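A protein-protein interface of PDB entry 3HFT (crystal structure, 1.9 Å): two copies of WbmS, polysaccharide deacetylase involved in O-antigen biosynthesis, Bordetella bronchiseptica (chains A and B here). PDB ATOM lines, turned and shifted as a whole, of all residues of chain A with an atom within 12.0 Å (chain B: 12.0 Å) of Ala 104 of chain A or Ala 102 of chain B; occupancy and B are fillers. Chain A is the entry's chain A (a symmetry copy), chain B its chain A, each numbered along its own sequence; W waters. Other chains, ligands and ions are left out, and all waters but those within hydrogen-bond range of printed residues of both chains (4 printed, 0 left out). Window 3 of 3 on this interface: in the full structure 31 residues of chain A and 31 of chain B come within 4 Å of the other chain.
Ala 104 of chain A touches one residue of chain B.
Of the printed residues of chain A, Ala 102 of chain B touches His 103, Ala 104 and Glu 105.
Of the printed residues of chain B, Gly 106 of chain A touches Leu 99 and Gly 101.
No residue of chain A comes within 4 Å of Ala 100 of chain B.
Of the printed residues of chain B, Leu 98 of chain A touches Leu 98.
Of the printed residues of chain B, Val 107 of chain A touches Leu 99.
Printed residues of chain B within 4 Å of Gly 101 of chain A: Glu 105 (3.5 Å) and Gly 106 (3.7 Å).
Of the printed residues of chain A, Ala 104 of chain B touches Ala 102 (3.2 Å).
Leu 111 of chain A touches none of the printed residues of chain B.
Phe 95 of chain B touches none of the printed residues of chain A.
The nearest printed residue of chain A that does not touch Gly 106 of chain B is Ala 100 of chain A (4.4 Å).
Leu 98 of chain A touches Leu 98 of chain B (CB to O, 3.7 Å).
Gly 106 of chain B touches Leu 99 of chain A (CA to O, 3.3 Å).
Gly 101 of chain A touches Glu 105 of chain B.
CA of Gly 101 of chain A touches N of Gly 106 of chain B, at 3.7 Å.
His 103 of chain B touches Ala 102 of chain A.
CB of Ala 102 of chain A touches O of Ala 104 of chain B, at 3.2 Å.
CB of Ala 102 of chain B touches O of Ala 104 of chain A, 3.2 Å away.
Glu 105 of chain A touches Gly 101 of chain B (O to O, 3.5 Å).
Ala 102 of chain B touches Glu 105 of chain A.
Gly 101 of chain B touches Gly 106 of chain A.
Leu 98 of chain A touches its own counterpart, Leu 98 of chain B.
Leu 99 of chain A touches Val 107 of chain B, and with the chains exchanged Val 107 of chain A touches Leu 99 of chain B.
Ala 102 of chain A touches His 103 of chain B, and with the chains exchanged His 103 of chain A touches Ala 102 of chain B.
Ala 102 of chain A touches Ala 104 of chain B, and with the chains exchanged Ala 104 of chain A touches Ala 102 of chain B.
Of the 16 pairs that touch across the chains among the printed residues, 16 have their exchanged pair printed and touching as well.
N of Val 107 of chain B is in hydrogen-bond range of O of Leu 99 of chain A.
The backbone carbonyl oxygen (O) of Leu 99 of chain B is in hydrogen-bond range of the backbone NH (N) of Val 107 of chain A (3.0 Å).
The backbone carbonyl oxygen (O) of His 103 of chain A lies within hydrogen-bond range of the backbone NH (N) of His 103 of chain B (2.9 Å).
A ring nitrogen (ND1) of His 103 of chain B sits at hydrogen-bond distance from the backbone NH of Glu 105 of chain B, 2.9 Å away.
N of Gly 106 of chain A sits at hydrogen-bond distance from OE1 of Glu 109 of chain A (3.0 Å).
The backbone NH (N) of Glu 105 of chain A is in hydrogen-bond range of a ring nitrogen (ND1) of His 103 of chain A, at 2.9 Å.
The side-chain carboxylate (OE1) of Glu 105 of chain B is in salt-bridge range of the guanidinium group (NH2) of Arg 113 of chain B (2.9 Å).
OE1 of Glu 105 of chain A is in salt-bridge range of NH2 of Arg 113 of chain A (2.9 Å).
Of the 20 printed residues of chain A, 9 touch a printed residue of chain B.
Along chain A the printed residues that touch a printed residue of chain B span positions 98 to 107.
Of the 16 printed residues of chain B, 9 touch a printed residue of chain A.
Hydrophobic or aromatic side chains of chain B within 4 Å of the printed part of chain A: Leu 98, Leu 99, Ala 102 and Val 107.
Among the printed residues, 16 pairs touch across the chains.
Among the printed residues, no Asp or Glu carboxylate lies within 4 Å of a Lys or Arg side-chain nitrogen of the other chain.
Water W2 lies within hydrogen-bond range of the side-chain carboxylate (OE1) of Glu 109 of chain A (2.7 Å), the backbone carbonyl oxygen (O) of Ala 100 of chain B (3.4 Å) and the backbone NH (N) of Gly 106 of chain A (3.4 Å).
Water W4 lies within hydrogen-bond range of the backbone carbonyl oxygen (O) of Leu 99 of chain B, the backbone NH (N) of Gln 108 of chain A and the backbone NH (N) of Val 107 of chain A.
Water W1 bridges O of Leu 99 of chain A and N of Val 107 of chain B.
Water W3 bridges O of Ala 100 of chain A and N of Gly 106 of chain B.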
ATOM      1  N   ASN A  94      13.137  15.308   9.558  1.00  0.00           N
ATOM      2  CA  ASN A  94      14.343  14.631   9.995  1.00  0.00           C
ATOM      3  C   ASN A  94      14.983  15.283  11.199  1.00  0.00           C
ATOM      4  O   ASN A  94      15.666  16.326  11.077  1.00  0.00           O
ATOM      5  CB  ASN A  94      15.364  14.614   8.876  1.00  0.00           C
ATOM      6  CG  ASN A  94      16.610  13.838   9.250  1.00  0.00           C
ATOM      7  OD1 ASN A  94      16.617  13.026  10.186  1.00  0.00           O
ATOM      8  ND2 ASN A  94      17.657  14.053   8.492  1.00  0.00           N
ATOM      9  N   PHE A  95      14.758  14.678  12.367  1.00  0.00           N
ATOM     10  CA  PHE A  95      15.286  15.207  13.609  1.00  0.00           C
ATOM     11  C   PHE A  95      16.564  14.504  14.054  1.00  0.00           C
ATOM     12  O   PHE A  95      17.104  14.853  15.105  1.00  0.00           O
ATOM     13  CB  PHE A  95      14.255  15.095  14.735  1.00  0.00           C
ATOM     14  CG  PHE A  95      12.910  15.728  14.429  1.00  0.00           C
ATOM     15  CD1 PHE A  95      12.796  17.092  14.190  1.00  0.00           C
ATOM     16  CD2 PHE A  95      11.747  14.953  14.448  1.00  0.00           C
ATOM     17  CE1 PHE A  95      11.550  17.679  13.930  1.00  0.00           C
ATOM     18  CE2 PHE A  95      10.498  15.537  14.214  1.00  0.00           C
ATOM     19  CZ  PHE A  95      10.397  16.899  13.945  1.00  0.00           C
ATOM     20  N   ASN A  96      17.079  13.581  13.243  1.00  0.00           N
ATOM     21  CA  ASN A  96      18.306  12.854  13.576  1.00  0.00           C
ATOM     22  C   ASN A  96      19.491  13.745  13.905  1.00  0.00           C
ATOM     23  O   ASN A  96      20.222  13.467  14.846  1.00  0.00           O
ATOM     24  CB  ASN A  96      18.703  11.860  12.462  1.00  0.00           C
ATOM     25  CG  ASN A  96      17.941  10.557  12.538  1.00  0.00           C
ATOM     26  OD1 ASN A  96      17.338  10.225  13.573  1.00  0.00           O
ATOM     27  ND2 ASN A  96      17.968   9.790  11.436  1.00  0.00           N
ATOM     28  N   PRO A  97      19.696  14.826  13.152  1.00  0.00           N
ATOM     29  CA  PRO A  97      20.839  15.690  13.516  1.00  0.00           C
ATOM     30  C   PRO A  97      20.802  16.215  14.956  1.00  0.00           C
ATOM     31  O   PRO A  97      21.832  16.541  15.531  1.00  0.00           O
ATOM     32  CB  PRO A  97      20.726  16.847  12.522  1.00  0.00           C
ATOM     33  CG  PRO A  97      19.997  16.234  11.333  1.00  0.00           C
ATOM     34  CD  PRO A  97      19.002  15.308  11.942  1.00  0.00           C
ATOM     35  N   LEU A  98      19.616  16.276  15.549  1.00  0.00           N
ATOM     36  CA  LEU A  98      19.499  16.743  16.914  1.00  0.00           C
ATOM     37  C   LEU A  98      20.066  15.704  17.878  1.00  0.00           C
ATOM     38  O   LEU A  98      20.582  16.035  18.952  1.00  0.00           O
ATOM     39  CB  LEU A  98      18.040  17.035  17.248  1.00  0.00           C
ATOM     40  CG  LEU A  98      17.314  18.035  16.345  1.00  0.00           C
ATOM     41  CD1 LEU A  98      15.875  18.172  16.823  1.00  0.00           C
ATOM     42  CD2 LEU A  98      18.006  19.383  16.317  1.00  0.00           C
ATOM     43  N   LEU A  99      19.966  14.446  17.484  1.00  0.00           N
ATOM     44  CA  LEU A  99      20.387  13.332  18.324  1.00  0.00           C
ATOM     45  C   LEU A  99      21.852  12.975  18.078  1.00  0.00           C
ATOM     46  O   LEU A  99      22.542  12.449  18.967  1.00  0.00           O
ATOM     47  CB  LEU A  99      19.538  12.108  18.005  1.00  0.00           C
ATOM     48  CG  LEU A  99      18.024  12.316  18.021  1.00  0.00           C
ATOM     49  CD1 LEU A  99      17.345  10.971  17.688  1.00  0.00           C
ATOM     50  CD2 LEU A  99      17.597  12.864  19.350  1.00  0.00           C
ATOM     51  N   ALA A 100      22.317  13.301  16.878  1.00  0.00           N
ATOM     52  CA  ALA A 100      23.655  12.928  16.409  1.00  0.00           C
ATOM     53  C   ALA A 100      24.825  13.565  17.134  1.00  0.00           C
ATOM     54  O   ALA A 100      25.912  12.999  17.156  1.00  0.00           O
ATOM     55  CB  ALA A 100      23.771  13.209  14.897  1.00  0.00           C
ATOM     56  N   GLY A 101      24.620  14.745  17.692  1.00  0.00           N
ATOM     57  CA  GLY A 101      25.673  15.455  18.377  1.00  0.00           C
ATOM     58  C   GLY A 101      25.282  16.910  18.442  1.00  0.00           C
ATOM     59  O   GLY A 101      24.125  17.248  18.214  1.00  0.00           O
ATOM     60  N   ALA A 102      26.242  17.788  18.719  1.00  0.00           N
ATOM     61  CA  ALA A 102      25.930  19.195  18.876  1.00  0.00           C
ATOM     62  C   ALA A 102      25.192  19.727  17.649  1.00  0.00           C
ATOM     63  O   ALA A 102      25.448  19.300  16.531  1.00  0.00           O
ATOM     64  CB  ALA A 102      27.219  20.012  19.136  1.00  0.00           C
ATOM     65  N   HIS A 103      24.255  20.647  17.872  1.00  0.00           N
ATOM     66  CA  HIS A 103      23.441  21.205  16.785  1.00  0.00           C
ATOM     67  C   HIS A 103      22.968  22.596  17.189  1.00  0.00           C
ATOM     68  O   HIS A 103      22.847  22.891  18.376  1.00  0.00           O
ATOM     69  CB  HIS A 103      22.235  20.294  16.507  1.00  0.00           C
ATOM     70  CG  HIS A 103      21.591  20.512  15.170  1.00  0.00           C
ATOM     71  ND1 HIS A 103      20.654  21.496  14.941  1.00  0.00           N
ATOM     72  CD2 HIS A 103      21.724  19.847  14.001  1.00  0.00           C
ATOM     73  CE1 HIS A 103      20.249  21.438  13.687  1.00  0.00           C
ATOM     74  NE2 HIS A 103      20.884  20.447  13.093  1.00  0.00           N
ATOM     75  N   ALA A 104      22.683  23.433  16.194  1.00  0.00           N
ATOM     76  CA  ALA A 104      22.267  24.831  16.416  1.00  0.00           C
ATOM     77  C   ALA A 104      20.766  25.053  16.579  1.00  0.00           C
ATOM     78  O   ALA A 104      20.337  26.129  16.989  1.00  0.00           O
ATOM     79  CB  ALA A 104      22.784  25.690  15.251  1.00  0.00           C
ATOM     80  N   GLU A 105      19.969  24.033  16.278  1.00  0.00           N
ATOM     81  CA  GLU A 105      18.522  24.159  16.261  1.00  0.00           C
ATOM     82  C   GLU A 105      17.866  23.082  17.079  1.00  0.00           C
ATOM     83  O   GLU A 105      18.523  22.156  17.506  1.00  0.00           O
ATOM     84  CB  GLU A 105      18.005  23.929  14.854  1.00  0.00           C
ATOM     85  CG  GLU A 105      18.485  24.904  13.861  1.00  0.00           C
ATOM     86  CD  GLU A 105      17.855  24.660  12.533  1.00  0.00           C
ATOM     87  OE1 GLU A 105      17.640  23.486  12.193  1.00  0.00           O
ATOM     88  OE2 GLU A 105      17.570  25.655  11.845  1.00  0.00           O
ATOM     89  N   GLY A 106      16.556  23.215  17.253  1.00  0.00           N
ATOM     90  CA  GLY A 106      15.737  22.168  17.869  1.00  0.00           C
ATOM     91  C   GLY A 106      14.691  21.650  16.893  1.00  0.00           C
ATOM     92  O   GLY A 106      14.748  21.895  15.677  1.00  0.00           O
ATOM     93  N   VAL A 107      13.727  20.930  17.445  1.00  0.00           N
ATOM     94  CA  VAL A 107      12.650  20.353  16.674  1.00  0.00           C
ATOM     95  C   VAL A 107      11.860  21.415  15.891  1.00  0.00           C
ATOM     96  O   VAL A 107      11.574  21.225  14.717  1.00  0.00           O
ATOM     97  CB  VAL A 107      11.705  19.513  17.598  1.00  0.00           C
ATOM     98  CG1 VAL A 107      10.351  19.293  16.948  1.00  0.00           C
ATOM     99  CG2 VAL A 107      12.381  18.158  17.963  1.00  0.00           C
ATOM    100  N   GLN A 108      11.534  22.528  16.538  1.00  0.00           N
ATOM    101  CA  GLN A 108      10.654  23.528  15.944  1.00  0.00           C
ATOM    102  C   GLN A 108      11.107  24.026  14.580  1.00  0.00           C
ATOM    103  O   GLN A 108      10.313  24.082  13.638  1.00  0.00           O
ATOM    104  CB  GLN A 108      10.474  24.710  16.899  1.00  0.00           C
ATOM    105  CG  GLN A 108       9.585  25.809  16.331  1.00  0.00           C
ATOM    106  N   GLU A 109      12.379  24.399  14.479  1.00  0.00           N
ATOM    107  CA  GLU A 109      12.917  24.920  13.239  1.00  0.00           C
ATOM    108  C   GLU A 109      12.823  23.872  12.145  1.00  0.00           C
ATOM    109  O   GLU A 109      12.408  24.184  11.022  1.00  0.00           O
ATOM    110  CB  GLU A 109      14.374  25.354  13.398  1.00  0.00           C
ATOM    111  CG  GLU A 109      14.600  26.555  14.328  1.00  0.00           C
ATOM    112  CD  GLU A 109      14.843  26.181  15.783  1.00  0.00           C
ATOM    113  OE1 GLU A 109      14.499  25.055  16.207  1.00  0.00           O
ATOM    114  OE2 GLU A 109      15.376  27.038  16.521  1.00  0.00           O
ATOM    115  N   ILE A 110      13.195  22.635  12.474  1.00  0.00           N
ATOM    116  CA  ILE A 110      13.186  21.548  11.483  1.00  0.00           C
ATOM    117  C   ILE A 110      11.757  21.205  11.016  1.00  0.00           C
ATOM    118  O   ILE A 110      11.509  20.995   9.822  1.00  0.00           O
ATOM    119  CB  ILE A 110      13.913  20.273  12.027  1.00  0.00           C
ATOM    120  CG1 ILE A 110      15.425  20.520  12.198  1.00  0.00           C
ATOM    121  CG2 ILE A 110      13.679  19.066  11.100  1.00  0.00           C
ATOM    122  CD1 ILE A 110      16.153  19.446  13.007  1.00  0.00           C
ATOM    123  N   LEU A 111      10.837  21.137  11.970  1.00  0.00           N
ATOM    124  CA  LEU A 111       9.445  20.826  11.693  1.00  0.00           C
ATOM    125  C   LEU A 111       8.821  21.898  10.831  1.00  0.00           C
ATOM    126  O   LEU A 111       8.139  21.592   9.866  1.00  0.00           O
ATOM    127  CB  LEU A 111       8.652  20.703  12.999  1.00  0.00           C
ATOM    128  CG  LEU A 111       7.131  20.457  12.934  1.00  0.00           C
ATOM    129  CD1 LEU A 111       6.774  19.172  12.081  1.00  0.00           C
ATOM    130  CD2 LEU A 111       6.508  20.386  14.376  1.00  0.00           C
ATOM    131  N   ARG A 113      10.302  24.026   8.836  1.00  0.00           N
ATOM    132  CA  ARG A 113      10.854  23.963   7.493  1.00  0.00           C
ATOM    133  C   ARG A 113      10.250  22.836   6.687  1.00  0.00           C
ATOM    134  O   ARG A 113       9.947  23.011   5.523  1.00  0.00           O
ATOM    135  CB  ARG A 113      12.365  23.782   7.503  1.00  0.00           C
ATOM    136  CG  ARG A 113      13.144  25.050   7.500  1.00  0.00           C
ATOM    137  CD  ARG A 113      14.542  24.787   6.975  1.00  0.00           C
ATOM    138  NE  ARG A 113      15.263  23.806   7.777  1.00  0.00           N
ATOM    139  CZ  ARG A 113      15.854  24.073   8.941  1.00  0.00           C
ATOM    140  NH1 ARG A 113      15.791  25.275   9.458  1.00  0.00           N
ATOM    141  NH2 ARG A 113      16.490  23.116   9.604  1.00  0.00           N
ATOM    142  N   MET A 138       4.054  19.528  19.529  1.00  0.00           N
ATOM    143  CA  MET A 138       4.362  20.487  18.495  1.00  0.00           C
ATOM    144  C   MET A 138       3.703  20.121  17.168  1.00  0.00           C
ATOM    145  O   MET A 138       3.322  21.014  16.401  1.00  0.00           O
ATOM    146  CB  MET A 138       5.880  20.659  18.342  1.00  0.00           C
ATOM    147  CG  MET A 138       6.519  21.518  19.463  1.00  0.00           C
ATOM    148  SD  MET A 138       8.346  22.027  19.042  1.00  0.00           S
ATOM    149  CE  MET A 138       8.138  21.853  17.209  1.00  0.00           C
ATOM    150  N   ASN B  94      17.335  11.737  29.983  1.00  0.00           N
ATOM    151  CA  ASN B  94      16.626  12.920  29.532  1.00  0.00           C
ATOM    152  C   ASN B  94      17.234  13.536  28.293  1.00  0.00           C
ATOM    153  O   ASN B  94      18.269  14.238  28.368  1.00  0.00           O
ATOM    154  CB  ASN B  94      16.623  13.970  30.623  1.00  0.00           C
ATOM    155  CG  ASN B  94      15.817  15.194  30.237  1.00  0.00           C
ATOM    156  OD1 ASN B  94      14.979  15.161  29.324  1.00  0.00           O
ATOM    157  ND2 ASN B  94      16.035  16.265  30.959  1.00  0.00           N
ATOM    158  N   PHE B  95      16.601  13.269  27.150  1.00  0.00           N
ATOM    159  CA  PHE B  95      17.088  13.771  25.879  1.00  0.00           C
ATOM    160  C   PHE B  95      16.351  15.025  25.419  1.00  0.00           C
ATOM    161  O   PHE B  95      16.663  15.540  24.344  1.00  0.00           O
ATOM    162  CB  PHE B  95      16.961  12.707  24.786  1.00  0.00           C
ATOM    163  CG  PHE B  95      17.625  11.381  25.110  1.00  0.00           C
ATOM    164  CD1 PHE B  95      18.997  11.296  25.314  1.00  0.00           C
ATOM    165  CD2 PHE B  95      16.869  10.206  25.144  1.00  0.00           C
ATOM    166  CE1 PHE B  95      19.611  10.067  25.592  1.00  0.00           C
ATOM    167  CE2 PHE B  95      17.480   8.974  25.396  1.00  0.00           C
ATOM    168  CZ  PHE B  95      18.851   8.902  25.630  1.00  0.00           C
ATOM    169  N   ASN B  96      15.443  15.547  26.241  1.00  0.00           N
ATOM    170  CA  ASN B  96      14.686  16.753  25.895  1.00  0.00           C
ATOM    171  C   ASN B  96      15.549  17.942  25.509  1.00  0.00           C
ATOM    172  O   ASN B  96      15.233  18.643  24.556  1.00  0.00           O
ATOM    173  CB  ASN B  96      13.717  17.165  27.025  1.00  0.00           C
ATOM    174  CG  ASN B  96      12.425  16.381  27.006  1.00  0.00           C
ATOM    175  OD1 ASN B  96      12.075  15.744  25.998  1.00  0.00           O
ATOM    176  ND2 ASN B  96      11.688  16.426  28.128  1.00  0.00           N
ATOM    177  N   PRO B  97      16.646  18.185  26.226  1.00  0.00           N
ATOM    178  CA  PRO B  97      17.480  19.331  25.807  1.00  0.00           C
ATOM    179  C   PRO B  97      17.967  19.262  24.354  1.00  0.00           C
ATOM    180  O   PRO B  97      18.259  20.281  23.743  1.00  0.00           O
ATOM    181  CB  PRO B  97      18.666  19.264  26.771  1.00  0.00           C
ATOM    182  CG  PRO B  97      18.098  18.559  27.996  1.00  0.00           C
ATOM    183  CD  PRO B  97      17.172  17.533  27.440  1.00  0.00           C
ATOM    184  N   LEU B  98      18.030  18.061  23.792  1.00  0.00           N
ATOM    185  CA  LEU B  98      18.462  17.914  22.418  1.00  0.00           C
ATOM    186  C   LEU B  98      17.388  18.438  21.469  1.00  0.00           C
ATOM    187  O   LEU B  98      17.681  18.928  20.372  1.00  0.00           O
ATOM    188  CB  LEU B  98      18.769  16.451  22.117  1.00  0.00           C
ATOM    189  CG  LEU B  98      19.806  15.766  23.011  1.00  0.00           C
ATOM    190  CD1 LEU B  98      19.953  14.317  22.569  1.00  0.00           C
ATOM    191  CD2 LEU B  98      21.142  16.480  22.983  1.00  0.00           C
ATOM    192  N   LEU B  99      16.143  18.329  21.900  1.00  0.00           N
ATOM    193  CA  LEU B  99      14.999  18.708  21.080  1.00  0.00           C
ATOM    194  C   LEU B  99      14.625  20.174  21.296  1.00  0.00           C
ATOM    195  O   LEU B  99      14.064  20.830  20.403  1.00  0.00           O
ATOM    196  CB  LEU B  99      13.800  17.849  21.457  1.00  0.00           C
ATOM    197  CG  LEU B  99      14.032  16.339  21.476  1.00  0.00           C
ATOM    198  CD1 LEU B  99      12.708  15.648  21.865  1.00  0.00           C
ATOM    199  CD2 LEU B  99      14.550  15.884  20.144  1.00  0.00           C
ATOM    200  N   ALA B 100      14.976  20.677  22.473  1.00  0.00           N
ATOM    201  CA  ALA B 100      14.594  22.021  22.916  1.00  0.00           C
ATOM    202  C   ALA B 100      15.192  23.181  22.142  1.00  0.00           C
ATOM    203  O   ALA B 100      14.607  24.257  22.105  1.00  0.00           O
ATOM    204  CB  ALA B 100      14.914  22.184  24.416  1.00  0.00           C
ATOM    205  N   GLY B 101      16.359  22.979  21.556  1.00  0.00           N
ATOM    206  CA  GLY B 101      17.032  24.024  20.823  1.00  0.00           C
ATOM    207  C   GLY B 101      18.492  23.654  20.729  1.00  0.00           C
ATOM    208  O   GLY B 101      18.855  22.509  20.979  1.00  0.00           O
ATOM    209  N   ALA B 102      19.345  24.620  20.401  1.00  0.00           N
ATOM    210  CA  ALA B 102      20.752  24.326  20.214  1.00  0.00           C
ATOM    211  C   ALA B 102      21.330  23.631  21.445  1.00  0.00           C
ATOM    212  O   ALA B 102      20.930  23.911  22.567  1.00  0.00           O
ATOM    213  CB  ALA B 102      21.541  25.619  19.896  1.00  0.00           C
ATOM    214  N   HIS B 103      22.259  22.703  21.223  1.00  0.00           N
ATOM    215  CA  HIS B 103      22.860  21.928  22.315  1.00  0.00           C
ATOM    216  C   HIS B 103      24.247  21.466  21.886  1.00  0.00           C
ATOM    217  O   HIS B 103      24.512  21.316  20.695  1.00  0.00           O
ATOM    218  CB  HIS B 103      21.977  20.716  22.652  1.00  0.00           C
ATOM    219  CG  HIS B 103      22.242  20.113  23.999  1.00  0.00           C
ATOM    220  ND1 HIS B 103      23.247  19.198  24.226  1.00  0.00           N
ATOM    221  CD2 HIS B 103      21.608  20.268  25.182  1.00  0.00           C
ATOM    222  CE1 HIS B 103      23.230  18.828  25.492  1.00  0.00           C
ATOM    223  NE2 HIS B 103      22.246  19.463  26.095  1.00  0.00           N
ATOM    224  N   ALA B 104      25.115  21.223  22.865  1.00  0.00           N
ATOM    225  CA  ALA B 104      26.514  20.822  22.615  1.00  0.00           C
ATOM    226  C   ALA B 104      26.756  19.321  22.487  1.00  0.00           C
ATOM    227  O   ALA B 104      27.827  18.898  22.060  1.00  0.00           O
ATOM    228  CB  ALA B 104      27.395  21.385  23.741  1.00  0.00           C
ATOM    229  N   GLU B 105      25.758  18.516  22.838  1.00  0.00           N
ATOM    230  CA  GLU B 105      25.908  17.073  22.892  1.00  0.00           C
ATOM    231  C   GLU B 105      24.820  16.378  22.122  1.00  0.00           C
ATOM    232  O   GLU B 105      23.873  17.008  21.703  1.00  0.00           O
ATOM    233  CB  GLU B 105      25.725  16.592  24.318  1.00  0.00           C
ATOM    234  CG  GLU B 105      26.719  17.114  25.270  1.00  0.00           C
ATOM    235  CD  GLU B 105      26.522  16.518  26.622  1.00  0.00           C
ATOM    236  OE1 GLU B 105      25.361  16.294  26.999  1.00  0.00           O
ATOM    237  OE2 GLU B 105      27.540  16.268  27.288  1.00  0.00           O
ATOM    238  N   GLY B 106      24.970  15.065  21.980  1.00  0.00           N
ATOM    239  CA  GLY B 106      23.920  14.213  21.416  1.00  0.00           C
ATOM    240  C   GLY B 106      23.447  13.186  22.434  1.00  0.00           C
ATOM    241  O   GLY B 106      23.724  13.281  23.642  1.00  0.00           O
ATOM    242  N   VAL B 107      22.728  12.196  21.929  1.00  0.00           N
ATOM    243  CA  VAL B 107      22.190  11.132  22.745  1.00  0.00           C
ATOM    244  C   VAL B 107      23.287  10.381  23.520  1.00  0.00           C
ATOM    245  O   VAL B 107      23.134  10.125  24.707  1.00  0.00           O
ATOM    246  CB  VAL B 107      21.341  10.149  21.871  1.00  0.00           C
ATOM    247  CG1 VAL B 107      21.161   8.810  22.565  1.00  0.00           C
ATOM    248  CG2 VAL B 107      19.966  10.793  21.526  1.00  0.00           C
ATOM    249  N   ILE B 110      24.578  11.830  26.864  1.00  0.00           N
ATOM    250  CA  ILE B 110      23.518  11.831  27.885  1.00  0.00           C
ATOM    251  C   ILE B 110      23.211  10.410  28.400  1.00  0.00           C
ATOM    252  O   ILE B 110      23.039  10.193  29.606  1.00  0.00           O
ATOM    253  CB  ILE B 110      22.216  12.523  27.356  1.00  0.00           C
ATOM    254  CG1 ILE B 110      22.434  14.033  27.137  1.00  0.00           C
ATOM    255  CG2 ILE B 110      21.040  12.296  28.323  1.00  0.00           C
ATOM    256  CD1 ILE B 110      21.326  14.721  26.339  1.00  0.00           C
ATOM    257  N   ARG B 113      26.115   9.061  30.539  1.00  0.00           N
ATOM    258  CA  ARG B 113      26.080   9.650  31.868  1.00  0.00           C
ATOM    259  C   ARG B 113      24.985   9.050  32.721  1.00  0.00           C
ATOM    260  O   ARG B 113      25.197   8.783  33.888  1.00  0.00           O
ATOM    261  CB  ARG B 113      25.874  11.157  31.821  1.00  0.00           C
ATOM    262  CG  ARG B 113      27.128  11.956  31.769  1.00  0.00           C
ATOM    263  CD  ARG B 113      26.856  13.363  32.262  1.00  0.00           C
ATOM    264  NE  ARG B 113      25.842  14.046  31.468  1.00  0.00           N
ATOM    265  CZ  ARG B 113      26.067  14.608  30.281  1.00  0.00           C
ATOM    266  NH1 ARG B 113      27.255  14.550  29.733  1.00  0.00           N
ATOM    267  NH2 ARG B 113      25.082  15.210  29.628  1.00  0.00           N
HETATM  268  O   HOH W   1      24.678  10.831  19.791  1.00  0.00           O
HETATM  269  O   HOH W   2      14.086  24.901  18.836  1.00  0.00           O
HETATM  270  O   HOH W   3      26.653  12.579  20.419  1.00  0.00           O
HETATM  271  O   HOH W   4      12.389  22.917  19.566  1.00  0.00           O
